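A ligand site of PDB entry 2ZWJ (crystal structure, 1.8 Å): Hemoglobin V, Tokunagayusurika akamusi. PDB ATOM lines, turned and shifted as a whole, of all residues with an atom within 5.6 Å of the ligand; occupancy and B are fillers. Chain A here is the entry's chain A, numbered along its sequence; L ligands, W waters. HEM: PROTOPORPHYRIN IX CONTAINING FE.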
ATOM      1  N   TYR A  35     -11.625 -17.149   0.095  1.00  0.00           N
ATOM      2  CA  TYR A  35     -13.056 -17.425  -0.120  1.00  0.00           C
ATOM      3  C   TYR A  35     -13.929 -16.206   0.219  1.00  0.00           C
ATOM      4  O   TYR A  35     -14.764 -15.786  -0.582  1.00  0.00           O
ATOM      5  CB  TYR A  35     -13.474 -18.619   0.730  1.00  0.00           C
ATOM      6  CG  TYR A  35     -14.963 -18.935   0.690  1.00  0.00           C
ATOM      7  CD1 TYR A  35     -15.582 -19.325  -0.500  1.00  0.00           C
ATOM      8  CD2 TYR A  35     -15.744 -18.879   1.856  1.00  0.00           C
ATOM      9  CE1 TYR A  35     -16.938 -19.619  -0.538  1.00  0.00           C
ATOM     10  CE2 TYR A  35     -17.095 -19.180   1.829  1.00  0.00           C
ATOM     11  CZ  TYR A  35     -17.688 -19.562   0.630  1.00  0.00           C
ATOM     12  OH  TYR A  35     -19.024 -19.875   0.586  1.00  0.00           O
ATOM     13  N   ASN A  42     -20.678 -14.065   1.693  1.00  0.00           N
ATOM     14  CA  ASN A  42     -20.621 -15.159   2.657  1.00  0.00           C
ATOM     15  C   ASN A  42     -20.178 -14.779   4.070  1.00  0.00           C
ATOM     16  O   ASN A  42     -20.527 -15.479   5.027  1.00  0.00           O
ATOM     17  CB  ASN A  42     -19.752 -16.292   2.096  1.00  0.00           C
ATOM     18  CG  ASN A  42     -20.378 -16.921   0.886  1.00  0.00           C
ATOM     19  OD1 ASN A  42     -21.434 -17.539   0.983  1.00  0.00           O
ATOM     20  ND2 ASN A  42     -19.750 -16.755  -0.272  1.00  0.00           N
ATOM     21  N   LYS A  45     -22.813 -14.732   6.848  1.00  0.00           N
ATOM     22  CA  LYS A  45     -23.375 -16.013   7.290  1.00  0.00           C
ATOM     23  C   LYS A  45     -22.794 -16.453   8.626  1.00  0.00           C
ATOM     24  O   LYS A  45     -23.403 -17.237   9.355  1.00  0.00           O
ATOM     25  CB  LYS A  45     -23.146 -17.108   6.241  1.00  0.00           C
ATOM     26  CG  LYS A  45     -23.647 -16.763   4.839  1.00  0.00           C
ATOM     27  CD  LYS A  45     -25.173 -16.687   4.783  1.00  0.00           C
ATOM     28  CE  LYS A  45     -25.672 -16.321   3.386  1.00  0.00           C
ATOM     29  NZ  LYS A  45     -25.055 -15.063   2.898  1.00  0.00           N
ATOM     30  N   PHE A  46     -21.606 -15.927   8.937  1.00  0.00           N
ATOM     31  CA  PHE A  46     -20.903 -16.242  10.174  1.00  0.00           C
ATOM     32  C   PHE A  46     -21.124 -15.110  11.160  1.00  0.00           C
ATOM     33  O   PHE A  46     -20.530 -14.037  11.036  1.00  0.00           O
ATOM     34  CB  PHE A  46     -19.402 -16.431   9.901  1.00  0.00           C
ATOM     35  CG  PHE A  46     -19.111 -17.507   8.900  1.00  0.00           C
ATOM     36  CD1 PHE A  46     -18.963 -18.829   9.319  1.00  0.00           C
ATOM     37  CD2 PHE A  46     -19.012 -17.203   7.545  1.00  0.00           C
ATOM     38  CE1 PHE A  46     -18.703 -19.842   8.381  1.00  0.00           C
ATOM     39  CE2 PHE A  46     -18.749 -18.203   6.606  1.00  0.00           C
ATOM     40  CZ  PHE A  46     -18.592 -19.526   7.029  1.00  0.00           C
ATOM     41  N   GLU A  47     -21.984 -15.356  12.135  1.00  0.00           N
ATOM     42  CA  GLU A  47     -22.373 -14.305  13.095  1.00  0.00           C
ATOM     43  C   GLU A  47     -21.197 -13.692  13.860  1.00  0.00           C
ATOM     44  O   GLU A  47     -21.239 -12.502  14.206  1.00  0.00           O
ATOM     45  CB  GLU A  47     -23.439 -14.820  14.050  1.00  0.00           C
ATOM     46  CG  GLU A  47     -24.771 -15.204  13.366  1.00  0.00           C
ATOM     47  CD  GLU A  47     -25.571 -14.000  12.868  1.00  0.00           C
ATOM     48  OE1 GLU A  47     -25.307 -12.864  13.296  1.00  0.00           O
ATOM     49  OE2 GLU A  47     -26.472 -14.206  12.033  1.00  0.00           O
ATOM     50  N   THR A  48     -20.161 -14.471  14.132  1.00  0.00           N
ATOM     51  CA  THR A  48     -18.993 -13.941  14.841  1.00  0.00           C
ATOM     52  C   THR A  48     -18.158 -12.982  13.993  1.00  0.00           C
ATOM     53  O   THR A  48     -17.374 -12.192  14.526  1.00  0.00           O
ATOM     54  CB  THR A  48     -18.083 -15.055  15.413  1.00  0.00           C
ATOM     55  OG1 THR A  48     -17.602 -15.894  14.340  1.00  0.00           O
ATOM     56  CG2 THR A  48     -18.834 -15.887  16.434  1.00  0.00           C
ATOM     57  N   ILE A  66     -12.975 -20.998  12.747  1.00  0.00           N
ATOM     58  CA  ILE A  66     -13.932 -21.341  11.689  1.00  0.00           C
ATOM     59  C   ILE A  66     -13.200 -21.996  10.519  1.00  0.00           C
ATOM     60  O   ILE A  66     -13.627 -23.048  10.049  1.00  0.00           O
ATOM     61  CB  ILE A  66     -14.753 -20.109  11.203  1.00  0.00           C
ATOM     62  CG1 ILE A  66     -15.574 -19.508  12.352  1.00  0.00           C
ATOM     63  CG2 ILE A  66     -15.652 -20.488  10.019  1.00  0.00           C
ATOM     64  CD1 ILE A  66     -16.217 -18.157  12.040  1.00  0.00           C
ATOM     65  N   ARG A  69     -12.001 -25.544  11.419  1.00  0.00           N
ATOM     66  CA  ARG A  69     -13.061 -26.560  11.521  1.00  0.00           C
ATOM     67  C   ARG A  69     -13.515 -27.071  10.161  1.00  0.00           C
ATOM     68  O   ARG A  69     -13.781 -28.273  10.011  1.00  0.00           O
ATOM     69  CB  ARG A  69     -14.228 -26.066  12.365  1.00  0.00           C
ATOM     70  CG  ARG A  69     -13.870 -25.960  13.843  1.00  0.00           C
ATOM     71  CD  ARG A  69     -15.057 -25.657  14.701  1.00  0.00           C
ATOM     72  NE  ARG A  69     -15.786 -26.860  15.108  1.00  0.00           N
ATOM     73  CZ  ARG A  69     -16.624 -26.904  16.136  1.00  0.00           C
ATOM     74  NH1 ARG A  69     -17.238 -28.039  16.435  1.00  0.00           N
ATOM     75  NH2 ARG A  69     -16.857 -25.824  16.878  1.00  0.00           N
ATOM     76  N   ILE A  70     -13.565 -26.185   9.154  1.00  0.00           N
ATOM     77  CA  ILE A  70     -13.820 -26.597   7.769  1.00  0.00           C
ATOM     78  C   ILE A  70     -12.757 -27.605   7.311  1.00  0.00           C
ATOM     79  O   ILE A  70     -13.072 -28.697   6.837  1.00  0.00           O
ATOM     80  CB  ILE A  70     -13.859 -25.378   6.792  1.00  0.00           C
ATOM     81  CG1 ILE A  70     -15.076 -24.495   7.069  1.00  0.00           C
ATOM     82  CG2 ILE A  70     -13.884 -25.853   5.332  1.00  0.00           C
ATOM     83  CD1 ILE A  70     -15.000 -23.110   6.412  1.00  0.00           C
ATOM     84  N   ILE A  73     -12.699 -31.152   8.955  1.00  0.00           N
ATOM     85  CA  ILE A  73     -13.664 -32.063   8.315  1.00  0.00           C
ATOM     86  C   ILE A  73     -13.079 -32.672   7.039  1.00  0.00           C
ATOM     87  O   ILE A  73     -13.105 -33.891   6.871  1.00  0.00           O
ATOM     88  CB  ILE A  73     -15.015 -31.377   8.001  1.00  0.00           C
ATOM     89  CG1 ILE A  73     -15.749 -30.967   9.288  1.00  0.00           C
ATOM     90  CG2 ILE A  73     -15.898 -32.290   7.095  1.00  0.00           C
ATOM     91  CD1 ILE A  73     -16.166 -32.139  10.240  1.00  0.00           C
ATOM     92  N   PHE A  74     -12.554 -31.831   6.148  1.00  0.00           N
ATOM     93  CA  PHE A  74     -11.956 -32.346   4.915  1.00  0.00           C
ATOM     94  C   PHE A  74     -10.792 -33.304   5.216  1.00  0.00           C
ATOM     95  O   PHE A  74     -10.658 -34.355   4.558  1.00  0.00           O
ATOM     96  CB  PHE A  74     -11.539 -31.217   3.969  1.00  0.00           C
ATOM     97  CG  PHE A  74     -12.700 -30.572   3.272  1.00  0.00           C
ATOM     98  CD1 PHE A  74     -13.539 -31.322   2.454  1.00  0.00           C
ATOM     99  CD2 PHE A  74     -12.972 -29.215   3.445  1.00  0.00           C
ATOM    100  CE1 PHE A  74     -14.634 -30.739   1.809  1.00  0.00           C
ATOM    101  CE2 PHE A  74     -14.058 -28.626   2.810  1.00  0.00           C
ATOM    102  CZ  PHE A  74     -14.887 -29.393   1.982  1.00  0.00           C
ATOM    103  N   MET A  94     -21.354 -33.395  10.571  1.00  0.00           N
ATOM    104  CA  MET A  94     -21.185 -31.955  10.326  1.00  0.00           C
ATOM    105  C   MET A  94     -22.372 -31.292   9.618  1.00  0.00           C
ATOM    106  O   MET A  94     -22.524 -30.078   9.677  1.00  0.00           O
ATOM    107  CB  MET A  94     -19.852 -31.631   9.640  1.00  0.00           C
ATOM    108  CG  MET A  94     -19.633 -32.228   8.246  1.00  0.00           C
ATOM    109  SD  MET A  94     -20.648 -31.556   6.895  1.00  0.00           S
ATOM    110  CE  MET A  94     -20.326 -29.814   7.058  1.00  0.00           C
ATOM    111  N   PRO A  97     -25.689 -28.944  11.858  1.00  0.00           N
ATOM    112  CA  PRO A  97     -25.625 -27.485  12.049  1.00  0.00           C
ATOM    113  C   PRO A  97     -25.851 -26.623  10.794  1.00  0.00           C
ATOM    114  O   PRO A  97     -26.073 -25.418  10.923  1.00  0.00           O
ATOM    115  CB  PRO A  97     -24.214 -27.243  12.614  1.00  0.00           C
ATOM    116  CG  PRO A  97     -23.788 -28.557  13.166  1.00  0.00           C
ATOM    117  CD  PRO A  97     -24.445 -29.596  12.313  1.00  0.00           C
ATOM    118  N   HIS A  98     -25.753 -27.207   9.599  1.00  0.00           N
ATOM    119  CA  HIS A  98     -25.984 -26.474   8.347  1.00  0.00           C
ATOM    120  C   HIS A  98     -27.406 -26.559   7.808  1.00  0.00           C
ATOM    121  O   HIS A  98     -27.788 -25.765   6.933  1.00  0.00           O
ATOM    122  CB  HIS A  98     -25.008 -26.937   7.265  1.00  0.00           C
ATOM    123  CG  HIS A  98     -23.576 -26.674   7.594  1.00  0.00           C
ATOM    124  ND1 HIS A  98     -22.807 -27.556   8.328  1.00  0.00           N
ATOM    125  CD2 HIS A  98     -22.765 -25.625   7.296  1.00  0.00           C
ATOM    126  CE1 HIS A  98     -21.590 -27.056   8.479  1.00  0.00           C
ATOM    127  NE2 HIS A  98     -21.539 -25.895   7.861  1.00  0.00           N
ATOM    128  N   ARG A 101     -29.575 -23.467   7.961  1.00  0.00           N
ATOM    129  CA  ARG A 101     -28.856 -22.264   7.521  1.00  0.00           C
ATOM    130  C   ARG A 101     -29.169 -21.832   6.092  1.00  0.00           C
ATOM    131  O   ARG A 101     -29.219 -22.674   5.179  1.00  0.00           O
ATOM    132  CB  ARG A 101     -27.353 -22.426   7.718  1.00  0.00           C
ATOM    133  CG  ARG A 101     -26.989 -22.826   9.144  1.00  0.00           C
ATOM    134  CD  ARG A 101     -25.593 -22.412   9.537  1.00  0.00           C
ATOM    135  NE  ARG A 101     -25.537 -22.192  10.984  1.00  0.00           N
ATOM    136  CZ  ARG A 101     -25.884 -21.054  11.592  1.00  0.00           C
ATOM    137  NH1 ARG A 101     -26.297 -20.000  10.887  1.00  0.00           N
ATOM    138  NH2 ARG A 101     -25.796 -20.966  12.904  1.00  0.00           N
ATOM    139  N   ILE A 103     -27.813 -21.000   3.361  1.00  0.00           N
ATOM    140  CA  ILE A 103     -26.609 -21.020   2.549  1.00  0.00           C
ATOM    141  C   ILE A 103     -26.925 -21.760   1.252  1.00  0.00           C
ATOM    142  O   ILE A 103     -27.436 -22.887   1.291  1.00  0.00           O
ATOM    143  CB  ILE A 103     -25.429 -21.693   3.302  1.00  0.00           C
ATOM    144  CG1 ILE A 103     -25.187 -20.970   4.645  1.00  0.00           C
ATOM    145  CG2 ILE A 103     -24.153 -21.689   2.450  1.00  0.00           C
ATOM    146  CD1 ILE A 103     -24.310 -21.728   5.605  1.00  0.00           C
ATOM    147  N   SER A 107     -22.869 -21.090  -2.803  1.00  0.00           N
ATOM    148  CA  SER A 107     -21.877 -20.743  -1.780  1.00  0.00           C
ATOM    149  C   SER A 107     -20.972 -21.923  -1.416  1.00  0.00           C
ATOM    150  O   SER A 107     -19.756 -21.774  -1.304  1.00  0.00           O
ATOM    151  CB  SER A 107     -22.571 -20.212  -0.512  1.00  0.00           C
ATOM    152  OG  SER A 107     -23.113 -18.926  -0.715  1.00  0.00           O
ATOM    153  N   TYR A 108     -21.581 -23.090  -1.239  1.00  0.00           N
ATOM    154  CA  TYR A 108     -20.840 -24.310  -0.922  1.00  0.00           C
ATOM    155  C   TYR A 108     -19.908 -24.673  -2.070  1.00  0.00           C
ATOM    156  O   TYR A 108     -18.729 -24.996  -1.864  1.00  0.00           O
ATOM    157  CB  TYR A 108     -21.788 -25.474  -0.635  1.00  0.00           C
ATOM    158  CG  TYR A 108     -22.574 -25.343   0.646  1.00  0.00           C
ATOM    159  CD1 TYR A 108     -21.918 -25.197   1.876  1.00  0.00           C
ATOM    160  CD2 TYR A 108     -23.959 -25.388   0.645  1.00  0.00           C
ATOM    161  CE1 TYR A 108     -22.633 -25.089   3.063  1.00  0.00           C
ATOM    162  CE2 TYR A 108     -24.686 -25.292   1.830  1.00  0.00           C
ATOM    163  CZ  TYR A 108     -24.015 -25.130   3.025  1.00  0.00           C
ATOM    164  OH  TYR A 108     -24.726 -25.024   4.199  1.00  0.00           O
ATOM    165  N   LEU A 111     -16.841 -22.496  -2.411  1.00  0.00           N
ATOM    166  CA  LEU A 111     -15.788 -22.888  -1.478  1.00  0.00           C
ATOM    167  C   LEU A 111     -15.004 -24.068  -2.038  1.00  0.00           C
ATOM    168  O   LEU A 111     -13.767 -24.055  -2.027  1.00  0.00           O
ATOM    169  CB  LEU A 111     -16.344 -23.198  -0.082  1.00  0.00           C
ATOM    170  CG  LEU A 111     -15.361 -23.801   0.934  1.00  0.00           C
ATOM    171  CD1 LEU A 111     -14.200 -22.848   1.249  1.00  0.00           C
ATOM    172  CD2 LEU A 111     -16.114 -24.201   2.198  1.00  0.00           C
ATOM    173  N   PHE A 136     -18.560 -36.228  -1.426  1.00  0.00           N
ATOM    174  CA  PHE A 136     -18.762 -35.288  -0.323  1.00  0.00           C
ATOM    175  C   PHE A 136     -20.075 -34.534  -0.493  1.00  0.00           C
ATOM    176  O   PHE A 136     -20.926 -34.549   0.399  1.00  0.00           O
ATOM    177  CB  PHE A 136     -17.589 -34.294  -0.206  1.00  0.00           C
ATOM    178  CG  PHE A 136     -17.741 -33.339   0.948  1.00  0.00           C
ATOM    179  CD1 PHE A 136     -17.098 -33.598   2.173  1.00  0.00           C
ATOM    180  CD2 PHE A 136     -18.532 -32.188   0.828  1.00  0.00           C
ATOM    181  CE1 PHE A 136     -17.237 -32.701   3.257  1.00  0.00           C
ATOM    182  CE2 PHE A 136     -18.671 -31.299   1.906  1.00  0.00           C
ATOM    183  CZ  PHE A 136     -18.027 -31.566   3.124  1.00  0.00           C
ATOM    184  N   PHE A 137     -20.227 -33.876  -1.641  1.00  0.00           N
ATOM    185  CA  PHE A 137     -21.426 -33.081  -1.900  1.00  0.00           C
ATOM    186  C   PHE A 137     -22.710 -33.887  -2.058  1.00  0.00           C
ATOM    187  O   PHE A 137     -23.763 -33.440  -1.598  1.00  0.00           O
ATOM    188  CB  PHE A 137     -21.185 -32.042  -3.008  1.00  0.00           C
ATOM    189  CG  PHE A 137     -20.381 -30.889  -2.515  1.00  0.00           C
ATOM    190  CD1 PHE A 137     -20.988 -29.853  -1.803  1.00  0.00           C
ATOM    191  CD2 PHE A 137     -18.993 -30.870  -2.659  1.00  0.00           C
ATOM    192  CE1 PHE A 137     -20.244 -28.808  -1.290  1.00  0.00           C
ATOM    193  CE2 PHE A 137     -18.237 -29.813  -2.144  1.00  0.00           C
ATOM    194  CZ  PHE A 137     -18.867 -28.782  -1.461  1.00  0.00           C
ATOM    195  N   PHE A 140     -23.546 -34.616   1.618  1.00  0.00           N
ATOM    196  CA  PHE A 140     -23.888 -33.354   2.247  1.00  0.00           C
ATOM    197  C   PHE A 140     -25.276 -32.863   1.837  1.00  0.00           C
ATOM    198  O   PHE A 140     -26.125 -32.605   2.690  1.00  0.00           O
ATOM    199  CB  PHE A 140     -22.811 -32.315   1.923  1.00  0.00           C
ATOM    200  CG  PHE A 140     -22.938 -31.039   2.685  1.00  0.00           C
ATOM    201  CD1 PHE A 140     -23.013 -31.041   4.078  1.00  0.00           C
ATOM    202  CD2 PHE A 140     -22.953 -29.816   2.015  1.00  0.00           C
ATOM    203  CE1 PHE A 140     -23.115 -29.847   4.786  1.00  0.00           C
ATOM    204  CE2 PHE A 140     -23.053 -28.609   2.722  1.00  0.00           C
ATOM    205  CZ  PHE A 140     -23.131 -28.624   4.116  1.00  0.00           C
HETATM  206  CHA HEM L   1     -20.285 -24.412  11.329  1.00  0.00           C
HETATM  207  CHB HEM L   1     -17.807 -27.443   8.462  1.00  0.00           C
HETATM  208  CHC HEM L   1     -19.228 -24.953   4.551  1.00  0.00           C
HETATM  209  CHD HEM L   1     -21.374 -21.696   7.423  1.00  0.00           C
HETATM  210  C1A HEM L   1     -19.455 -25.417  10.893  1.00  0.00           C
HETATM  211  C2A HEM L   1     -18.711 -26.329  11.743  1.00  0.00           C
HETATM  212  C3A HEM L   1     -18.015 -27.166  10.948  1.00  0.00           C
HETATM  213  C4A HEM L   1     -18.321 -26.818   9.578  1.00  0.00           C
HETATM  214  CMA HEM L   1     -17.079 -28.309  11.399  1.00  0.00           C
HETATM  215  CAA HEM L   1     -18.685 -26.297  13.298  1.00  0.00           C
HETATM  216  CBA HEM L   1     -19.974 -26.818  13.899  1.00  0.00           C
HETATM  217  CGA HEM L   1     -20.660 -25.703  14.664  1.00  0.00           C
HETATM  218  O1A HEM L   1     -20.139 -25.264  15.733  1.00  0.00           O
HETATM  219  O2A HEM L   1     -21.732 -25.278  14.208  1.00  0.00           O
HETATM  220  C1B HEM L   1     -17.998 -27.057   7.153  1.00  0.00           C
HETATM  221  C2B HEM L   1     -17.497 -27.742   5.982  1.00  0.00           C
HETATM  222  C3B HEM L   1     -17.902 -27.061   4.891  1.00  0.00           C
HETATM  223  C4B HEM L   1     -18.656 -25.911   5.345  1.00  0.00           C
HETATM  224  CMB HEM L   1     -16.668 -29.042   5.971  1.00  0.00           C
HETATM  225  CAB HEM L   1     -17.608 -27.411   3.418  1.00  0.00           C
HETATM  226  CBB HEM L   1     -18.639 -27.626   2.580  1.00  0.00           C
HETATM  227  C1C HEM L   1     -19.826 -23.794   4.993  1.00  0.00           C
HETATM  228  C2C HEM L   1     -20.107 -22.609   4.198  1.00  0.00           C
HETATM  229  C3C HEM L   1     -20.697 -21.708   5.003  1.00  0.00           C
HETATM  230  C4C HEM L   1     -20.816 -22.301   6.318  1.00  0.00           C
HETATM  231  CMC HEM L   1     -19.740 -22.462   2.698  1.00  0.00           C
HETATM  232  CAC HEM L   1     -21.213 -20.276   4.682  1.00  0.00           C
HETATM  233  CBC HEM L   1     -21.038 -19.664   3.495  1.00  0.00           C
HETATM  234  C1D HEM L   1     -21.343 -22.141   8.727  1.00  0.00           C
HETATM  235  C2D HEM L   1     -22.021 -21.503   9.826  1.00  0.00           C
HETATM  236  C3D HEM L   1     -21.680 -22.347  11.070  1.00  0.00           C
HETATM  237  C4D HEM L   1     -20.838 -23.412  10.564  1.00  0.00           C
HETATM  238  CMD HEM L   1     -22.883 -20.226   9.732  1.00  0.00           C
HETATM  239  CAD HEM L   1     -22.131 -22.173  12.556  1.00  0.00           C
HETATM  240  CBD HEM L   1     -22.025 -20.741  13.078  1.00  0.00           C
HETATM  241  CGD HEM L   1     -20.583 -20.335  13.210  1.00  0.00           C
HETATM  242  O1D HEM L   1     -19.893 -20.253  12.167  1.00  0.00           O
HETATM  243  O2D HEM L   1     -20.120 -20.060  14.352  1.00  0.00           O
HETATM  244  NA  HEM L   1     -19.193 -25.756   9.580  1.00  0.00           N
HETATM  245  NB  HEM L   1     -18.701 -25.949   6.723  1.00  0.00           N
HETATM  246  NC  HEM L   1     -20.270 -23.571   6.272  1.00  0.00           N
HETATM  247  ND  HEM L   1     -20.656 -23.258   9.198  1.00  0.00           N
HETATM  248 FE   HEM L   1     -19.755 -24.654   7.936  1.00  0.00          FE
HETATM  249  O   HOH W   1     -19.720 -17.476  13.302  1.00  0.00           O
HETATM  250  O   HOH W   2     -23.431 -24.845  10.604  1.00  0.00           O
HETATM  251  O   HOH W   3     -23.194 -17.926  12.273  1.00  0.00           O
HETATM  252  O   HOH W   4     -22.523 -17.969  15.274  1.00  0.00           O
HETATM  253  O   HOH W   5     -17.867 -23.386   8.377  1.00  0.00           O
HETATM  254  O   HOH W   6     -17.778 -22.408  13.216  1.00  0.00           O
HETATM  255  O   HOH W   7     -25.665 -18.618   8.534  1.00  0.00           O
HETATM  256  O   HOH W   8     -16.686 -23.590  11.212  1.00  0.00           O
HETATM  257  O   HOH W   9     -14.171 -29.658  12.441  1.00  0.00           O
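Water W1 lies within hydrogen-bond range of an oxygen (O2D) of the ligand (2.8 Å), the side-chain hydroxyl (OG1) of Thr 48 (2.8 Å) and the backbone NH (N) of Glu 47 (3.3 Å). Water W2 lies within hydrogen-bond range of O of Pro 97 (2.7 Å), NE of Arg 101 (3.4 Å) and N of His 98 (3.5 Å). Water W7 lies within hydrogen-bond range of O of Lys 45 (2.8 Å) and NH1 of Arg 101 (2.8 Å).
Merely in contact with the ligand: Lys 45 (3.1 Å), Asn 42 (3.3 Å), Phe 46 (3.3 Å), Tyr 35 (3.4 Å), Ile 103 (3.5 Å), Arg 101 (3.5 Å), Ile 73 (3.5 Å), Pro 97 (3.5 Å), Tyr 108 (3.6 Å), Met 94 (3.6 Å), Phe 74 (3.7 Å), Ile 70 (3.7 Å), Phe 136 (3.7 Å) and Leu 111 (3.7 Å). Hydrophobic or aromatic side chains that line the ligand: Phe 46, Ile 70, Ile 73, Phe 74, Met 94, Pro 97, His 98, Ile 103, Tyr 108, Leu 111 and Phe 136. Within 4 Å of the ligand: Tyr 35, Asn 42, Lys 45, Phe 46, Arg 69, Ile 70, Ile 73, Phe 74, Met 94, Pro 97, His 98, Arg 101, Ile 103, Tyr 108, Leu 111 and Phe 136.
A ring nitrogen (ND1) of His 98 is in hydrogen-bond range of the backbone carbonyl oxygen (O) of Met 94, at 2.9 Å. ND2 of Asn 42 sits close to OH of Tyr 35 (3.3 Å). The side-chain amide oxygen (OD1) of Asn 42 is in hydrogen-bond range of the side-chain hydroxyl (OG) of Ser 107. The side-chain hydroxyl (OH) of Tyr 35 lies within hydrogen-bond range of the backbone carbonyl oxygen (O) of Ser 107 (2.8 Å). The guanidinium group (NE) of Arg 101 sits at hydrogen-bond distance from the backbone carbonyl oxygen (O) of Pro 97 (3.3 Å).
FE of the ligand is bound by NE2 of His 98. An oxygen (O1A) of the ligand is in salt-bridge range of the guanidinium group (NH2) of Arg 69 (3.5 Å).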
